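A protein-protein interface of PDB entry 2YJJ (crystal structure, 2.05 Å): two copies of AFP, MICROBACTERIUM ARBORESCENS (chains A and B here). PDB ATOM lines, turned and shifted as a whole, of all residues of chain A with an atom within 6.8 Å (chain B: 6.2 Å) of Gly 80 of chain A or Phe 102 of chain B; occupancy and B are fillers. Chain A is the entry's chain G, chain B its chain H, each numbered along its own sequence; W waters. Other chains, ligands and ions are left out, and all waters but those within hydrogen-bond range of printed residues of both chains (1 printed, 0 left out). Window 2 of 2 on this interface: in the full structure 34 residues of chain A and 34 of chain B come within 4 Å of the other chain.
The backbone carbonyl oxygen (O) of Ile 83 of chain A is in hydrogen-bond range of the side-chain amide nitrogen (ND2) of Asn 45 of chain B.
O of Ile 83 of chain A sits close to O of Ala 100 of chain B, at 3.4 Å.
No position is printed for both chains.
Of the 12 pairs that touch across the chains among the printed residues, none has its exchanged pair printed and touching as well.
Gly 80 of chain A touches just one residue of chain B: Phe 102 (3.3 Å).
Phe 102 of chain B touches four residues of chain A.
Printed residues of chain B within 4 Å of Val 77 of chain A: Trp 44, Arg 47 and Phe 102.
Printed residues of chain A within 4 Å of Gly 101 of chain B: Pro 82 (3.7 Å).
Of the printed residues of chain A, Asn 45 of chain B touches Pro 82 (3.5 Å) and Ile 83 (3.2 Å).
Of the printed residues of chain A, Ala 100 of chain B touches Ile 83.
Of the printed residues of chain B, Pro 82 of chain A touches Asn 45, Gly 101 and Phe 102.
The nearest residue of chain B that does not touch Gly 80 of chain A is Arg 47 of chain B (5.4 Å).
The nearest printed residue of chain A that does not touch Arg 47 of chain B is Gly 80 of chain A (5.4 Å).
The backbone carbonyl oxygen (O) of Ile 76 of chain A sits at hydrogen-bond distance from the backbone NH (N) of Leu 81 of chain A, 3.4 Å away.
N of Ala 103 of chain B lies within hydrogen-bond range of O of Asn 45 of chain B, at 3.2 Å.
The backbone NH of Arg 47 of chain B is in hydrogen-bond range of the backbone carbonyl oxygen of Ala 103 of chain B, 2.9 Å away.
Leu 11 of chain A touches Arg 47 of chain B.
Val 77 of chain A touches Trp 44 of chain B.
CG1 of Val 77 of chain A touches NH2 of Arg 47 of chain B, at 3.9 Å.
CE1 of Phe 102 of chain B touches CG1 of Val 77 of chain A (3.8 Å).
Gly 80 of chain A touches Phe 102 of chain B.
Leu 81 of chain A touches Phe 102 of chain B (C to CZ, 3.3 Å).
Asn 45 of chain B touches Pro 82 of chain A.
Pro 82 of chain A touches Gly 101 of chain B (CB to CA, 3.7 Å).
Pro 82 of chain A touches Phe 102 of chain B.
CG2 of Ile 83 of chain A touches CB of Trp 44 of chain B, 3.96 Å away.
Water W1 lies within hydrogen-bond range of the guanidinium group (NH2) of Arg 47 of chain B (2.7 Å) and the backbone carbonyl oxygen (O) of Val 77 of chain A (2.7 Å).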
ATOM      1  N   LEU A  11     -22.585 -22.170  -6.551  1.00  0.00           N
ATOM      2  CA  LEU A  11     -21.915 -22.646  -7.806  1.00  0.00           C
ATOM      3  C   LEU A  11     -22.839 -23.234  -8.885  1.00  0.00           C
ATOM      4  O   LEU A  11     -22.815 -22.777 -10.034  1.00  0.00           O
ATOM      5  CB  LEU A  11     -20.675 -23.539  -7.569  1.00  0.00           C
ATOM      6  CG  LEU A  11     -19.290 -22.871  -7.351  1.00  0.00           C
ATOM      7  CD1 LEU A  11     -18.320 -23.887  -6.739  1.00  0.00           C
ATOM      8  CD2 LEU A  11     -18.700 -22.210  -8.606  1.00  0.00           C
ATOM      9  N   THR A  12     -23.630 -24.238  -8.525  1.00  0.00           N
ATOM     10  CA  THR A  12     -24.736 -24.665  -9.384  1.00  0.00           C
ATOM     11  C   THR A  12     -26.090 -24.202  -8.799  1.00  0.00           C
ATOM     12  O   THR A  12     -26.699 -24.898  -7.973  1.00  0.00           O
ATOM     13  CB  THR A  12     -24.640 -26.199  -9.867  1.00  0.00           C
ATOM     14  OG1 THR A  12     -25.946 -26.770 -10.059  1.00  0.00           O
ATOM     15  CG2 THR A  12     -23.713 -27.080  -8.987  1.00  0.00           C
ATOM     16  N   ALA A  13     -26.508 -22.999  -9.220  1.00  0.00           N
ATOM     17  CA  ALA A  13     -27.628 -22.269  -8.599  1.00  0.00           C
ATOM     18  C   ALA A  13     -28.976 -22.885  -8.931  1.00  0.00           C
ATOM     19  O   ALA A  13     -29.935 -22.792  -8.136  1.00  0.00           O
ATOM     20  CB  ALA A  13     -27.620 -20.816  -9.031  1.00  0.00           C
ATOM     21  N   ALA A  18     -29.147 -26.519 -14.972  1.00  0.00           N
ATOM     22  CA  ALA A  18     -27.820 -27.103 -15.249  1.00  0.00           C
ATOM     23  C   ALA A  18     -27.929 -28.446 -15.963  1.00  0.00           C
ATOM     24  O   ALA A  18     -27.241 -28.683 -16.971  1.00  0.00           O
ATOM     25  CB  ALA A  18     -26.951 -27.260 -13.950  1.00  0.00           C
ATOM     26  N   ARG A  75     -21.365 -22.470 -21.463  1.00  0.00           N
ATOM     27  CA  ARG A  75     -22.723 -22.422 -20.921  1.00  0.00           C
ATOM     28  C   ARG A  75     -23.032 -23.550 -19.936  1.00  0.00           C
ATOM     29  O   ARG A  75     -23.651 -23.305 -18.881  1.00  0.00           O
ATOM     30  CB  ARG A  75     -23.773 -22.367 -22.023  1.00  0.00           C
ATOM     31  CG  ARG A  75     -25.197 -22.354 -21.439  1.00  0.00           C
ATOM     32  CD  ARG A  75     -25.549 -20.952 -20.960  1.00  0.00           C
ATOM     33  NE  ARG A  75     -26.890 -20.966 -20.391  1.00  0.00           N
ATOM     34  CZ  ARG A  75     -27.325 -20.106 -19.500  1.00  0.00           C
ATOM     35  NH1 ARG A  75     -26.542 -19.088 -19.154  1.00  0.00           N
ATOM     36  NH2 ARG A  75     -28.576 -20.200 -19.061  1.00  0.00           N
ATOM     37  N   ILE A  76     -22.625 -24.776 -20.247  1.00  0.00           N
ATOM     38  CA  ILE A  76     -22.799 -25.875 -19.317  1.00  0.00           C
ATOM     39  C   ILE A  76     -22.066 -25.656 -18.001  1.00  0.00           C
ATOM     40  O   ILE A  76     -22.647 -25.792 -16.891  1.00  0.00           O
ATOM     41  CB  ILE A  76     -22.325 -27.221 -19.969  1.00  0.00           C
ATOM     42  CG1 ILE A  76     -23.107 -27.484 -21.240  1.00  0.00           C
ATOM     43  CG2 ILE A  76     -22.365 -28.369 -18.932  1.00  0.00           C
ATOM     44  CD1 ILE A  76     -22.512 -28.611 -22.079  1.00  0.00           C
ATOM     45  N   VAL A  77     -20.782 -25.369 -18.124  1.00  0.00           N
ATOM     46  CA  VAL A  77     -19.963 -25.099 -16.971  1.00  0.00           C
ATOM     47  C   VAL A  77     -20.426 -23.873 -16.148  1.00  0.00           C
ATOM     48  O   VAL A  77     -20.423 -23.945 -14.931  1.00  0.00           O
ATOM     49  CB  VAL A  77     -18.470 -24.993 -17.377  1.00  0.00           C
ATOM     50  CG1 VAL A  77     -17.653 -24.562 -16.222  1.00  0.00           C
ATOM     51  CG2 VAL A  77     -17.972 -26.341 -17.954  1.00  0.00           C
ATOM     52  N   ALA A  78     -20.829 -22.785 -16.776  1.00  0.00           N
ATOM     53  CA  ALA A  78     -21.333 -21.632 -16.023  1.00  0.00           C
ATOM     54  C   ALA A  78     -22.524 -22.010 -15.118  1.00  0.00           C
ATOM     55  O   ALA A  78     -22.763 -21.386 -14.077  1.00  0.00           O
ATOM     56  CB  ALA A  78     -21.743 -20.505 -16.944  1.00  0.00           C
ATOM     57  N   LEU A  79     -23.304 -22.989 -15.558  1.00  0.00           N
ATOM     58  CA  LEU A  79     -24.519 -23.415 -14.827  1.00  0.00           C
ATOM     59  C   LEU A  79     -24.168 -24.392 -13.720  1.00  0.00           C
ATOM     60  O   LEU A  79     -24.992 -24.705 -12.844  1.00  0.00           O
ATOM     61  CB  LEU A  79     -25.585 -23.973 -15.784  1.00  0.00           C
ATOM     62  CG  LEU A  79     -26.190 -22.905 -16.733  1.00  0.00           C
ATOM     63  CD1 LEU A  79     -27.197 -23.532 -17.667  1.00  0.00           C
ATOM     64  CD2 LEU A  79     -26.868 -21.779 -15.949  1.00  0.00           C
ATOM     65  N   GLY A  80     -22.948 -24.893 -13.750  1.00  0.00           N
ATOM     66  CA  GLY A  80     -22.370 -25.616 -12.614  1.00  0.00           C
ATOM     67  C   GLY A  80     -22.035 -27.084 -12.810  1.00  0.00           C
ATOM     68  O   GLY A  80     -21.712 -27.775 -11.875  1.00  0.00           O
ATOM     69  N   LEU A  81     -22.110 -27.606 -14.008  1.00  0.00           N
ATOM     70  CA  LEU A  81     -21.813 -29.039 -14.167  1.00  0.00           C
ATOM     71  C   LEU A  81     -20.607 -29.167 -15.070  1.00  0.00           C
ATOM     72  O   LEU A  81     -20.398 -28.314 -15.904  1.00  0.00           O
ATOM     73  CB  LEU A  81     -22.994 -29.772 -14.800  1.00  0.00           C
ATOM     74  CG  LEU A  81     -24.245 -30.032 -13.982  1.00  0.00           C
ATOM     75  CD1 LEU A  81     -25.256 -30.720 -14.821  1.00  0.00           C
ATOM     76  CD2 LEU A  81     -23.941 -30.873 -12.729  1.00  0.00           C
ATOM     77  N   PRO A  82     -19.790 -30.207 -14.878  1.00  0.00           N
ATOM     78  CA  PRO A  82     -18.591 -30.308 -15.718  1.00  0.00           C
ATOM     79  C   PRO A  82     -18.906 -30.823 -17.145  1.00  0.00           C
ATOM     80  O   PRO A  82     -20.018 -31.232 -17.432  1.00  0.00           O
ATOM     81  CB  PRO A  82     -17.716 -31.316 -14.975  1.00  0.00           C
ATOM     82  CG  PRO A  82     -18.715 -32.190 -14.253  1.00  0.00           C
ATOM     83  CD  PRO A  82     -19.793 -31.204 -13.790  1.00  0.00           C
ATOM     84  N   ILE A  83     -17.919 -30.815 -18.018  1.00  0.00           N
ATOM     85  CA  ILE A  83     -18.099 -31.356 -19.369  1.00  0.00           C
ATOM     86  C   ILE A  83     -16.931 -32.295 -19.609  1.00  0.00           C
ATOM     87  O   ILE A  83     -15.787 -31.893 -19.349  1.00  0.00           O
ATOM     88  CB  ILE A  83     -18.051 -30.171 -20.444  1.00  0.00           C
ATOM     89  CG1 ILE A  83     -17.977 -30.742 -21.834  1.00  0.00           C
ATOM     90  CG2 ILE A  83     -16.804 -29.236 -20.226  1.00  0.00           C
ATOM     91  CD1 ILE A  83     -19.308 -30.882 -22.531  1.00  0.00           C
ATOM     92  N   TRP B  44     -12.045 -25.252 -19.691  1.00  0.00           N
ATOM     93  CA  TRP B  44     -13.470 -25.214 -19.280  1.00  0.00           C
ATOM     94  C   TRP B  44     -13.648 -25.605 -17.822  1.00  0.00           C
ATOM     95  O   TRP B  44     -14.515 -25.086 -17.130  1.00  0.00           O
ATOM     96  CB  TRP B  44     -14.343 -26.131 -20.193  1.00  0.00           C
ATOM     97  CG  TRP B  44     -14.300 -25.574 -21.628  1.00  0.00           C
ATOM     98  CD1 TRP B  44     -14.210 -24.229 -22.000  1.00  0.00           C
ATOM     99  CD2 TRP B  44     -14.338 -26.310 -22.850  1.00  0.00           C
ATOM    100  NE1 TRP B  44     -14.290 -24.101 -23.374  1.00  0.00           N
ATOM    101  CE2 TRP B  44     -14.327 -25.356 -23.920  1.00  0.00           C
ATOM    102  CE3 TRP B  44     -14.429 -27.692 -23.157  1.00  0.00           C
ATOM    103  CZ2 TRP B  44     -14.375 -25.738 -25.278  1.00  0.00           C
ATOM    104  CZ3 TRP B  44     -14.499 -28.060 -24.486  1.00  0.00           C
ATOM    105  CH2 TRP B  44     -14.448 -27.101 -25.534  1.00  0.00           C
ATOM    106  N   ASN B  45     -12.871 -26.562 -17.381  1.00  0.00           N
ATOM    107  CA  ASN B  45     -13.175 -27.251 -16.112  1.00  0.00           C
ATOM    108  C   ASN B  45     -12.279 -26.820 -14.952  1.00  0.00           C
ATOM    109  O   ASN B  45     -12.387 -27.370 -13.878  1.00  0.00           O
ATOM    110  CB  ASN B  45     -13.015 -28.776 -16.303  1.00  0.00           C
ATOM    111  CG  ASN B  45     -14.087 -29.380 -17.147  1.00  0.00           C
ATOM    112  OD1 ASN B  45     -15.193 -29.575 -16.718  1.00  0.00           O
ATOM    113  ND2 ASN B  45     -13.752 -29.684 -18.390  1.00  0.00           N
ATOM    114  N   VAL B  46     -11.341 -25.909 -15.163  1.00  0.00           N
ATOM    115  CA  VAL B  46     -10.401 -25.495 -14.111  1.00  0.00           C
ATOM    116  C   VAL B  46     -11.174 -24.720 -13.049  1.00  0.00           C
ATOM    117  O   VAL B  46     -12.118 -23.992 -13.393  1.00  0.00           O
ATOM    118  CB  VAL B  46      -9.150 -24.754 -14.695  1.00  0.00           C
ATOM    119  CG1 VAL B  46      -9.528 -23.460 -15.561  1.00  0.00           C
ATOM    120  CG2 VAL B  46      -8.110 -24.442 -13.606  1.00  0.00           C
ATOM    121  N   ARG B  47     -10.782 -24.916 -11.783  1.00  0.00           N
ATOM    122  CA  ARG B  47     -11.379 -24.244 -10.597  1.00  0.00           C
ATOM    123  C   ARG B  47     -10.319 -23.765  -9.653  1.00  0.00           C
ATOM    124  O   ARG B  47      -9.188 -24.287  -9.675  1.00  0.00           O
ATOM    125  CB  ARG B  47     -12.111 -25.276  -9.769  1.00  0.00           C
ATOM    126  CG  ARG B  47     -12.924 -26.208 -10.604  1.00  0.00           C
ATOM    127  CD  ARG B  47     -14.355 -26.003 -10.255  1.00  0.00           C
ATOM    128  NE  ARG B  47     -14.948 -25.297 -11.325  1.00  0.00           N
ATOM    129  CZ  ARG B  47     -16.230 -24.986 -11.408  1.00  0.00           C
ATOM    130  NH1 ARG B  47     -17.104 -25.315 -10.429  1.00  0.00           N
ATOM    131  NH2 ARG B  47     -16.606 -24.332 -12.501  1.00  0.00           N
ATOM    132  N   PRO B  99      -8.118 -34.291 -16.336  1.00  0.00           N
ATOM    133  CA  PRO B  99      -9.232 -35.004 -15.716  1.00  0.00           C
ATOM    134  C   PRO B  99     -10.482 -34.868 -16.531  1.00  0.00           C
ATOM    135  O   PRO B  99     -10.662 -33.874 -17.261  1.00  0.00           O
ATOM    136  CB  PRO B  99      -9.427 -34.265 -14.363  1.00  0.00           C
ATOM    137  CG  PRO B  99      -8.085 -33.550 -14.087  1.00  0.00           C
ATOM    138  CD  PRO B  99      -7.414 -33.350 -15.416  1.00  0.00           C
ATOM    139  N   ALA B 100     -11.406 -35.784 -16.304  1.00  0.00           N
ATOM    140  CA  ALA B 100     -12.714 -35.780 -16.963  1.00  0.00           C
ATOM    141  C   ALA B 100     -13.675 -34.642 -16.543  1.00  0.00           C
ATOM    142  O   ALA B 100     -14.603 -34.309 -17.287  1.00  0.00           O
ATOM    143  CB  ALA B 100     -13.391 -37.121 -16.677  1.00  0.00           C
ATOM    144  N   GLY B 101     -13.551 -34.158 -15.323  1.00  0.00           N
ATOM    145  CA  GLY B 101     -14.445 -33.078 -14.842  1.00  0.00           C
ATOM    146  C   GLY B 101     -13.724 -31.893 -14.213  1.00  0.00           C
ATOM    147  O   GLY B 101     -12.571 -31.607 -14.560  1.00  0.00           O
ATOM    148  N   PHE B 102     -14.396 -31.204 -13.281  1.00  0.00           N
ATOM    149  CA  PHE B 102     -13.810 -30.118 -12.451  1.00  0.00           C
ATOM    150  C   PHE B 102     -12.520 -30.530 -11.738  1.00  0.00           C
ATOM    151  O   PHE B 102     -12.432 -31.584 -11.151  1.00  0.00           O
ATOM    152  CB  PHE B 102     -14.837 -29.560 -11.412  1.00  0.00           C
ATOM    153  CG  PHE B 102     -16.022 -28.867 -12.038  1.00  0.00           C
ATOM    154  CD1 PHE B 102     -15.906 -28.199 -13.266  1.00  0.00           C
ATOM    155  CD2 PHE B 102     -17.308 -28.922 -11.428  1.00  0.00           C
ATOM    156  CE1 PHE B 102     -17.035 -27.557 -13.884  1.00  0.00           C
ATOM    157  CE2 PHE B 102     -18.422 -28.300 -12.052  1.00  0.00           C
ATOM    158  CZ  PHE B 102     -18.279 -27.589 -13.275  1.00  0.00           C
ATOM    159  N   ALA B 103     -11.479 -29.703 -11.822  1.00  0.00           N
ATOM    160  CA  ALA B 103     -10.262 -29.992 -11.102  1.00  0.00           C
ATOM    161  C   ALA B 103      -9.654 -28.672 -10.708  1.00  0.00           C
ATOM    162  O   ALA B 103      -9.852 -27.668 -11.370  1.00  0.00           O
ATOM    163  CB  ALA B 103      -9.274 -30.817 -12.048  1.00  0.00           C
ATOM    164  N   GLN B 104      -8.920 -28.686  -9.617  1.00  0.00           N
ATOM    165  CA  GLN B 104      -8.189 -27.520  -9.135  1.00  0.00           C
ATOM    166  C   GLN B 104      -7.096 -27.149 -10.118  1.00  0.00           C
ATOM    167  O   GLN B 104      -6.584 -27.975 -10.842  1.00  0.00           O
ATOM    168  CB  GLN B 104      -7.621 -27.825  -7.771  1.00  0.00           C
ATOM    169  CG  GLN B 104      -8.720 -27.963  -6.664  1.00  0.00           C
ATOM    170  CD  GLN B 104      -9.455 -26.646  -6.448  1.00  0.00           C
ATOM    171  OE1 GLN B 104     -10.675 -26.577  -6.574  1.00  0.00           O
ATOM    172  NE2 GLN B 104      -8.704 -25.596  -6.177  1.00  0.00           N
ATOM    173  N   GLU B 108      -4.824 -29.280 -13.127  1.00  0.00           N
ATOM    174  CA  GLU B 108      -4.872 -29.043 -14.582  1.00  0.00           C
ATOM    175  C   GLU B 108      -3.442 -28.692 -15.061  1.00  0.00           C
ATOM    176  O   GLU B 108      -3.008 -29.168 -16.082  1.00  0.00           O
ATOM    177  CB  GLU B 108      -5.844 -27.911 -14.953  1.00  0.00           C
ATOM    178  CG  GLU B 108      -7.277 -28.136 -14.399  1.00  0.00           C
ATOM    179  CD  GLU B 108      -8.053 -29.161 -15.250  1.00  0.00           C
ATOM    180  OE1 GLU B 108      -7.412 -29.853 -16.040  1.00  0.00           O
ATOM    181  OE2 GLU B 108      -9.294 -29.283 -15.149  1.00  0.00           O
HETATM  182  O   HOH W   1     -19.268 -23.801 -12.448  1.00  0.00           O
